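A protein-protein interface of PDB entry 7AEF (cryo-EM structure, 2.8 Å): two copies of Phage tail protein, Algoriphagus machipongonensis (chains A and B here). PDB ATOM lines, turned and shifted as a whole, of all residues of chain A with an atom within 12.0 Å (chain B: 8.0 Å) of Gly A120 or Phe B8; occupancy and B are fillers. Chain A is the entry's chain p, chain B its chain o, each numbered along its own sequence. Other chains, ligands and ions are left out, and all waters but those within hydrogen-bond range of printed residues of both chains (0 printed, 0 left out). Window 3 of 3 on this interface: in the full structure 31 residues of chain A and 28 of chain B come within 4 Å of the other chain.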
ATOM      1  N   THR A  64      -3.966  30.165  -6.930  1.00  0.00           N
ATOM      2  CA  THR A  64      -3.351  30.409  -5.619  1.00  0.00           C
ATOM      3  C   THR A  64      -1.874  30.030  -5.529  1.00  0.00           C
ATOM      4  O   THR A  64      -1.485  28.915  -5.862  1.00  0.00           O
ATOM      5  CB  THR A  64      -4.147  29.659  -4.527  1.00  0.00           C
ATOM      6  OG1 THR A  64      -5.485  30.144  -4.507  1.00  0.00           O
ATOM      7  CG2 THR A  64      -3.540  29.883  -3.155  1.00  0.00           C
ATOM      8  N   THR A 116     -11.379  28.666  -2.943  1.00  0.00           N
ATOM      9  CA  THR A 116     -11.581  27.372  -3.564  1.00  0.00           C
ATOM     10  C   THR A 116     -12.247  26.331  -2.705  1.00  0.00           C
ATOM     11  O   THR A 116     -12.267  26.425  -1.478  1.00  0.00           O
ATOM     12  CB  THR A 116     -10.226  26.786  -3.938  1.00  0.00           C
ATOM     13  OG1 THR A 116      -9.429  26.616  -2.760  1.00  0.00           O
ATOM     14  CG2 THR A 116      -9.581  27.676  -4.808  1.00  0.00           C
ATOM     15  N   ASP A 117     -12.734  25.282  -3.371  1.00  0.00           N
ATOM     16  CA  ASP A 117     -13.344  24.118  -2.718  1.00  0.00           C
ATOM     17  C   ASP A 117     -12.304  22.993  -2.721  1.00  0.00           C
ATOM     18  O   ASP A 117     -11.494  22.927  -3.624  1.00  0.00           O
ATOM     19  CB  ASP A 117     -14.659  23.698  -3.376  1.00  0.00           C
ATOM     20  CG  ASP A 117     -14.509  23.355  -4.839  1.00  0.00           C
ATOM     21  OD1 ASP A 117     -13.377  23.221  -5.325  1.00  0.00           O
ATOM     22  OD2 ASP A 117     -15.532  23.215  -5.517  1.00  0.00           O
ATOM     23  N   LEU A 118     -12.310  22.136  -1.703  1.00  0.00           N
ATOM     24  CA  LEU A 118     -11.319  21.094  -1.528  1.00  0.00           C
ATOM     25  C   LEU A 118     -11.930  19.728  -1.772  1.00  0.00           C
ATOM     26  O   LEU A 118     -13.020  19.446  -1.284  1.00  0.00           O
ATOM     27  CB  LEU A 118     -10.769  21.201  -0.106  1.00  0.00           C
ATOM     28  CG  LEU A 118     -10.159  22.592   0.282  1.00  0.00           C
ATOM     29  CD1 LEU A 118      -9.821  22.598   1.741  1.00  0.00           C
ATOM     30  CD2 LEU A 118      -8.918  22.878  -0.534  1.00  0.00           C
ATOM     31  N   LYS A 119     -11.231  18.874  -2.519  1.00  0.00           N
ATOM     32  CA  LYS A 119     -11.722  17.528  -2.799  1.00  0.00           C
ATOM     33  C   LYS A 119     -10.632  16.472  -2.688  1.00  0.00           C
ATOM     34  O   LYS A 119      -9.520  16.670  -3.170  1.00  0.00           O
ATOM     35  CB  LYS A 119     -12.324  17.473  -4.197  1.00  0.00           C
ATOM     36  CG  LYS A 119     -13.539  18.325  -4.392  1.00  0.00           C
ATOM     37  CD  LYS A 119     -14.097  18.168  -5.779  1.00  0.00           C
ATOM     38  CE  LYS A 119     -15.325  19.033  -5.964  1.00  0.00           C
ATOM     39  NZ  LYS A 119     -15.880  18.936  -7.337  1.00  0.00           N
ATOM     40  N   GLY A 120     -10.974  15.319  -2.109  1.00  0.00           N
ATOM     41  CA  GLY A 120     -10.049  14.190  -1.943  1.00  0.00           C
ATOM     42  C   GLY A 120      -9.478  13.660  -3.256  1.00  0.00           C
ATOM     43  O   GLY A 120      -8.334  13.214  -3.308  1.00  0.00           O
ATOM     44  N   ASP A 121     -10.272  13.709  -4.312  1.00  0.00           N
ATOM     45  CA  ASP A 121      -9.899  13.286  -5.642  1.00  0.00           C
ATOM     46  C   ASP A 121      -9.821  14.470  -6.614  1.00  0.00           C
ATOM     47  O   ASP A 121      -9.879  14.314  -7.839  1.00  0.00           O
ATOM     48  CB  ASP A 121     -10.865  12.201  -6.080  1.00  0.00           C
ATOM     49  CG  ASP A 121     -12.291  12.663  -6.001  1.00  0.00           C
ATOM     50  OD1 ASP A 121     -12.522  13.696  -5.380  1.00  0.00           O
ATOM     51  OD2 ASP A 121     -13.152  11.998  -6.517  1.00  0.00           O
ATOM     52  N   GLY A 122      -9.634  15.664  -6.068  1.00  0.00           N
ATOM     53  CA  GLY A 122      -9.572  16.893  -6.837  1.00  0.00           C
ATOM     54  C   GLY A 122      -8.245  17.127  -7.516  1.00  0.00           C
ATOM     55  O   GLY A 122      -7.473  17.989  -7.105  1.00  0.00           O
ATOM     56  N   ASN A 123      -7.985  16.384  -8.570  1.00  0.00           N
ATOM     57  CA  ASN A 123      -6.718  16.495  -9.293  1.00  0.00           C
ATOM     58  C   ASN A 123      -6.670  17.731 -10.200  1.00  0.00           C
ATOM     59  O   ASN A 123      -6.675  17.604 -11.422  1.00  0.00           O
ATOM     60  CB  ASN A 123      -6.489  15.251 -10.128  1.00  0.00           C
ATOM     61  CG  ASN A 123      -5.105  15.153 -10.681  1.00  0.00           C
ATOM     62  OD1 ASN A 123      -4.147  15.608 -10.056  1.00  0.00           O
ATOM     63  ND2 ASN A 123      -4.976  14.579 -11.840  1.00  0.00           N
ATOM     64  N   GLU A 124      -6.626  18.921  -9.590  1.00  0.00           N
ATOM     65  CA  GLU A 124      -6.640  20.189 -10.333  1.00  0.00           C
ATOM     66  C   GLU A 124      -5.960  21.333  -9.549  1.00  0.00           C
ATOM     67  O   GLU A 124      -5.555  21.152  -8.403  1.00  0.00           O
ATOM     68  CB  GLU A 124      -8.131  20.486 -10.672  1.00  0.00           C
ATOM     69  CG  GLU A 124      -8.505  21.780 -11.468  1.00  0.00           C
ATOM     70  CD  GLU A 124      -7.855  21.919 -12.828  1.00  0.00           C
ATOM     71  OE1 GLU A 124      -8.471  21.645 -13.825  1.00  0.00           O
ATOM     72  OE2 GLU A 124      -6.717  22.297 -12.832  1.00  0.00           O
ATOM     73  N   VAL A 125      -5.870  22.506 -10.170  1.00  0.00           N
ATOM     74  CA  VAL A 125      -5.312  23.728  -9.594  1.00  0.00           C
ATOM     75  C   VAL A 125      -6.325  24.481  -8.752  1.00  0.00           C
ATOM     76  O   VAL A 125      -7.473  24.661  -9.150  1.00  0.00           O
ATOM     77  CB  VAL A 125      -4.802  24.675 -10.704  1.00  0.00           C
ATOM     78  CG1 VAL A 125      -4.312  26.012 -10.119  1.00  0.00           C
ATOM     79  CG2 VAL A 125      -3.698  24.017 -11.447  1.00  0.00           C
ATOM     80  N   ALA A 126      -5.899  24.932  -7.587  1.00  0.00           N
ATOM     81  CA  ALA A 126      -6.756  25.728  -6.732  1.00  0.00           C
ATOM     82  C   ALA A 126      -6.864  27.168  -7.274  1.00  0.00           C
ATOM     83  O   ALA A 126      -5.850  27.867  -7.343  1.00  0.00           O
ATOM     84  CB  ALA A 126      -6.172  25.714  -5.329  1.00  0.00           C
ATOM     85  N   ILE A 127      -8.076  27.575  -7.693  1.00  0.00           N
ATOM     86  CA  ILE A 127      -8.324  28.901  -8.281  1.00  0.00           C
ATOM     87  C   ILE A 127      -9.172  29.823  -7.419  1.00  0.00           C
ATOM     88  O   ILE A 127     -10.325  29.529  -7.143  1.00  0.00           O
ATOM     89  CB  ILE A 127      -9.078  28.780  -9.647  1.00  0.00           C
ATOM     90  CG1 ILE A 127      -8.315  27.881 -10.670  1.00  0.00           C
ATOM     91  CG2 ILE A 127      -9.376  30.192 -10.264  1.00  0.00           C
ATOM     92  CD1 ILE A 127      -6.936  28.344 -11.084  1.00  0.00           C
ATOM     93  N   LEU B   5      -0.427  26.040  -6.121  1.00  0.00           N
ATOM     94  CA  LEU B   5      -0.776  24.959  -5.205  1.00  0.00           C
ATOM     95  C   LEU B   5      -1.889  24.066  -5.764  1.00  0.00           C
ATOM     96  O   LEU B   5      -2.789  24.543  -6.462  1.00  0.00           O
ATOM     97  CB  LEU B   5      -1.257  25.596  -3.893  1.00  0.00           C
ATOM     98  CG  LEU B   5      -0.232  26.475  -3.103  1.00  0.00           C
ATOM     99  CD1 LEU B   5      -0.955  27.204  -1.991  1.00  0.00           C
ATOM    100  CD2 LEU B   5       0.844  25.603  -2.502  1.00  0.00           C
ATOM    101  N   SER B   6      -1.853  22.780  -5.412  1.00  0.00           N
ATOM    102  CA  SER B   6      -2.899  21.809  -5.745  1.00  0.00           C
ATOM    103  C   SER B   6      -4.022  21.886  -4.714  1.00  0.00           C
ATOM    104  O   SER B   6      -3.898  22.594  -3.720  1.00  0.00           O
ATOM    105  CB  SER B   6      -2.330  20.406  -5.825  1.00  0.00           C
ATOM    106  OG  SER B   6      -1.930  19.953  -4.570  1.00  0.00           O
ATOM    107  N   LYS B   7      -5.121  21.151  -4.941  1.00  0.00           N
ATOM    108  CA  LYS B   7      -6.299  21.245  -4.027  1.00  0.00           C
ATOM    109  C   LYS B   7      -6.680  19.932  -3.317  1.00  0.00           C
ATOM    110  O   LYS B   7      -7.798  19.904  -2.765  1.00  0.00           O
ATOM    111  CB  LYS B   7      -7.505  21.784  -4.804  1.00  0.00           C
ATOM    112  CG  LYS B   7      -7.934  20.947  -6.002  1.00  0.00           C
ATOM    113  CD  LYS B   7      -9.104  21.540  -6.757  1.00  0.00           C
ATOM    114  CE  LYS B   7     -10.342  21.701  -5.902  1.00  0.00           C
ATOM    115  NZ  LYS B   7     -11.468  22.286  -6.669  1.00  0.00           N
ATOM    116  N   PHE B   8      -5.826  18.903  -3.280  1.00  0.00           N
ATOM    117  CA  PHE B   8      -6.253  17.655  -2.629  1.00  0.00           C
ATOM    118  C   PHE B   8      -5.626  17.265  -1.282  1.00  0.00           C
ATOM    119  O   PHE B   8      -6.054  16.283  -0.685  1.00  0.00           O
ATOM    120  CB  PHE B   8      -6.094  16.490  -3.611  1.00  0.00           C
ATOM    121  CG  PHE B   8      -4.711  16.279  -4.115  1.00  0.00           C
ATOM    122  CD1 PHE B   8      -3.790  15.547  -3.397  1.00  0.00           C
ATOM    123  CD2 PHE B   8      -4.329  16.806  -5.327  1.00  0.00           C
ATOM    124  CE1 PHE B   8      -2.527  15.357  -3.873  1.00  0.00           C
ATOM    125  CE2 PHE B   8      -3.063  16.612  -5.804  1.00  0.00           C
ATOM    126  CZ  PHE B   8      -2.163  15.888  -5.075  1.00  0.00           C
ATOM    127  N   HIS B   9      -4.628  17.984  -0.789  1.00  0.00           N
ATOM    128  CA  HIS B   9      -4.011  17.609   0.486  1.00  0.00           C
ATOM    129  C   HIS B   9      -4.327  18.672   1.552  1.00  0.00           C
ATOM    130  O   HIS B   9      -3.826  19.798   1.483  1.00  0.00           O
ATOM    131  CB  HIS B   9      -2.510  17.430   0.273  1.00  0.00           C
ATOM    132  CG  HIS B   9      -1.718  16.926   1.422  1.00  0.00           C
ATOM    133  ND1 HIS B   9      -0.397  17.217   1.549  1.00  0.00           N
ATOM    134  CD2 HIS B   9      -2.021  16.126   2.471  1.00  0.00           C
ATOM    135  CE1 HIS B   9       0.085  16.657   2.612  1.00  0.00           C
ATOM    136  NE2 HIS B   9      -0.867  15.977   3.209  1.00  0.00           N
ATOM    137  N   PHE B  10      -5.198  18.326   2.495  1.00  0.00           N
ATOM    138  CA  PHE B  10      -5.694  19.275   3.497  1.00  0.00           C
ATOM    139  C   PHE B  10      -6.173  18.590   4.772  1.00  0.00           C
ATOM    140  O   PHE B  10      -6.381  17.378   4.785  1.00  0.00           O
ATOM    141  CB  PHE B  10      -6.842  20.106   2.889  1.00  0.00           C
ATOM    142  CG  PHE B  10      -8.050  19.299   2.453  1.00  0.00           C
ATOM    143  CD1 PHE B  10      -9.126  19.093   3.307  1.00  0.00           C
ATOM    144  CD2 PHE B  10      -8.102  18.739   1.188  1.00  0.00           C
ATOM    145  CE1 PHE B  10     -10.206  18.345   2.908  1.00  0.00           C
ATOM    146  CE2 PHE B  10      -9.180  17.993   0.792  1.00  0.00           C
ATOM    147  CZ  PHE B  10     -10.241  17.793   1.655  1.00  0.00           C
ATOM    148  N   SER B  11      -6.393  19.376   5.830  1.00  0.00           N
ATOM    149  CA  SER B  11      -6.959  18.849   7.079  1.00  0.00           C
ATOM    150  C   SER B  11      -7.920  19.818   7.781  1.00  0.00           C
ATOM    151  O   SER B  11      -7.836  21.043   7.628  1.00  0.00           O
ATOM    152  CB  SER B  11      -5.856  18.495   8.038  1.00  0.00           C
ATOM    153  OG  SER B  11      -5.148  19.626   8.433  1.00  0.00           O
ATOM    154  N   PHE B  21     -11.429  14.539   5.754  1.00  0.00           N
ATOM    155  CA  PHE B  21     -12.684  14.824   5.065  1.00  0.00           C
ATOM    156  C   PHE B  21     -12.580  14.574   3.586  1.00  0.00           C
ATOM    157  O   PHE B  21     -11.497  14.635   3.011  1.00  0.00           O
ATOM    158  CB  PHE B  21     -13.157  16.258   5.350  1.00  0.00           C
ATOM    159  CG  PHE B  21     -13.625  16.468   6.763  1.00  0.00           C
ATOM    160  CD1 PHE B  21     -12.761  16.632   7.814  1.00  0.00           C
ATOM    161  CD2 PHE B  21     -14.971  16.514   7.027  1.00  0.00           C
ATOM    162  CE1 PHE B  21     -13.230  16.805   9.086  1.00  0.00           C
ATOM    163  CE2 PHE B  21     -15.433  16.701   8.306  1.00  0.00           C
ATOM    164  CZ  PHE B  21     -14.563  16.839   9.327  1.00  0.00           C
ATOM    165  N   THR B  22     -13.714  14.296   2.976  1.00  0.00           N
ATOM    166  CA  THR B  22     -13.819  14.095   1.546  1.00  0.00           C
ATOM    167  C   THR B  22     -13.967  15.425   0.815  1.00  0.00           C
ATOM    168  O   THR B  22     -13.372  15.636  -0.240  1.00  0.00           O
ATOM    169  CB  THR B  22     -14.982  13.124   1.203  1.00  0.00           C
ATOM    170  OG1 THR B  22     -14.720  11.816   1.760  1.00  0.00           O
ATOM    171  CG2 THR B  22     -15.136  12.988  -0.266  1.00  0.00           C
ATOM    172  N   GLU B  23     -14.781  16.317   1.365  1.00  0.00           N
ATOM    173  CA  GLU B  23     -15.058  17.588   0.708  1.00  0.00           C
ATOM    174  C   GLU B  23     -15.311  18.741   1.674  1.00  0.00           C
ATOM    175  O   GLU B  23     -15.952  18.573   2.714  1.00  0.00           O
ATOM    176  CB  GLU B  23     -16.262  17.436  -0.219  1.00  0.00           C
ATOM    177  CG  GLU B  23     -16.612  18.659  -1.048  1.00  0.00           C
ATOM    178  CD  GLU B  23     -17.794  18.441  -1.955  1.00  0.00           C
ATOM    179  OE1 GLU B  23     -18.219  17.314  -2.120  1.00  0.00           O
ATOM    180  OE2 GLU B  23     -18.291  19.398  -2.481  1.00  0.00           O
ATOM    181  N   VAL B  24     -14.768  19.916   1.333  1.00  0.00           N
ATOM    182  CA  VAL B  24     -14.975  21.161   2.078  1.00  0.00           C
ATOM    183  C   VAL B  24     -15.377  22.298   1.121  1.00  0.00           C
ATOM    184  O   VAL B  24     -14.665  22.556   0.152  1.00  0.00           O
ATOM    185  CB  VAL B  24     -13.678  21.580   2.825  1.00  0.00           C
ATOM    186  CG1 VAL B  24     -13.896  22.898   3.605  1.00  0.00           C
ATOM    187  CG2 VAL B  24     -13.225  20.466   3.756  1.00  0.00           C
ATOM    188  N   LEU B  92      -4.597  24.003   4.304  1.00  0.00           N
ATOM    189  CA  LEU B  92      -3.992  23.460   3.073  1.00  0.00           C
ATOM    190  C   LEU B  92      -2.547  23.108   3.399  1.00  0.00           C
ATOM    191  O   LEU B  92      -1.813  23.954   3.924  1.00  0.00           O
ATOM    192  CB  LEU B  92      -4.073  24.502   1.949  1.00  0.00           C
ATOM    193  CG  LEU B  92      -3.639  24.090   0.524  1.00  0.00           C
ATOM    194  CD1 LEU B  92      -4.389  24.959  -0.469  1.00  0.00           C
ATOM    195  CD2 LEU B  92      -2.122  24.308   0.341  1.00  0.00           C
ATOM    196  N   LEU B  93      -2.143  21.869   3.095  1.00  0.00           N
ATOM    197  CA  LEU B  93      -0.822  21.352   3.479  1.00  0.00           C
ATOM    198  C   LEU B  93       0.254  21.215   2.393  1.00  0.00           C
ATOM    199  O   LEU B  93      -0.041  21.014   1.218  1.00  0.00           O
ATOM    200  CB  LEU B  93      -1.046  19.971   4.082  1.00  0.00           C
ATOM    201  CG  LEU B  93      -2.017  19.888   5.284  1.00  0.00           C
ATOM    202  CD1 LEU B  93      -2.218  18.456   5.633  1.00  0.00           C
ATOM    203  CD2 LEU B  93      -1.480  20.656   6.468  1.00  0.00           C
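The backbone NH (N) of Leu B5 sits at hydrogen-bond distance from the backbone carbonyl oxygen (O) of Thr A64 (3.1 Å). N of Ala A126 lies within hydrogen-bond range of O of Leu B5, at 3.3 Å. NZ of Lys B7 lies within salt-bridge range of OD1 of Asp A117. The backbone NH (N) of Lys B7 sits close to the backbone carbonyl oxygen (O) of Glu A124 (3.5 Å). The backbone carbonyl oxygen of Thr B22 is in hydrogen-bond range of the backbone NH of Gly A120, 3.1 Å away. The backbone carbonyl oxygen (O) of Val B24 is in hydrogen-bond range of the backbone NH (N) of Leu A118, 3.0 Å away.
The backbone NH (N) of Thr A64 lies within hydrogen-bond range of the backbone carbonyl oxygen (O) of Ala A126, at 3.0 Å.
Asp A117 touches Val B24 (CA to O, 3.5 Å). Phe B10 touches Leu A118 (CE2 to CB, 3.7 Å). O of Leu A118 touches O of Thr B22, 3.97 Å away. CA of Glu B23 touches O of Leu A118 (3.4 Å). N of Lys A119 touches CE2 of Phe B10, at 3.99 Å. Lys A119 touches Thr B22 (CA to O, 3.6 Å). O of Gly A120 touches CB of Phe B8 (3.98 Å). Gly A122 touches Lys B7. O of Gly A122 touches CD2 of Phe B8, at 3.8 Å. Ser B6 touches Glu A124.
Printed residues of chain B within 4 Å of Asp A117: Lys B7 and Val B24. Of the printed residues of chain B, Gly A120 touches Phe B8 and Thr B22. Printed residues of chain A within 4 Å of Leu B5: Thr A64 (3.1 Å) and Ala A126 (3.3 Å). Ser B6 touches one residue of chain A. Printed residues of chain A within 4 Å of Lys B7: Asp A117, Leu A118, Lys A119, Gly A122 and Glu A124. Of the printed residues of chain A, Phe B8 touches Lys A119, Gly A120 and Gly A122. Phe B21 touches none of the printed residues of chain A. Thr B22 touches three residues of chain A. Leu B92 touches none of the printed residues of chain A. The nearest printed residue of chain B that does not touch Gly A120 is Phe B10 (4.3 Å). The nearest printed residue of chain A that does not touch Phe B8 is Asn A123 (4.5 Å). The nearest printed residue of chain B that does not touch Ala A126 is Ser B6 (4.2 Å).
Of the 13 printed residues of chain B, 8 touch a printed residue of chain A. Printed residues of chain B that touch a printed residue of chain A: Leu B5, Ser B6, Lys B7, Phe B8, Phe B10, Thr B22, Glu B23 and Val B24. Hydrophobic or aromatic side chains of chain B within 4 Å of the printed part of chain A: Leu B5, Phe B8 and Phe B10. Hydrophobic or aromatic side chains of chain A that line the printed part of chain B: Leu A118 and Ala A126. Among the printed residues, Asp or Glu carboxylates within 4 Å of a Lys or Arg side-chain nitrogen of the other chain: Asp A117 with Lys B7.
No position is printed for both chains.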
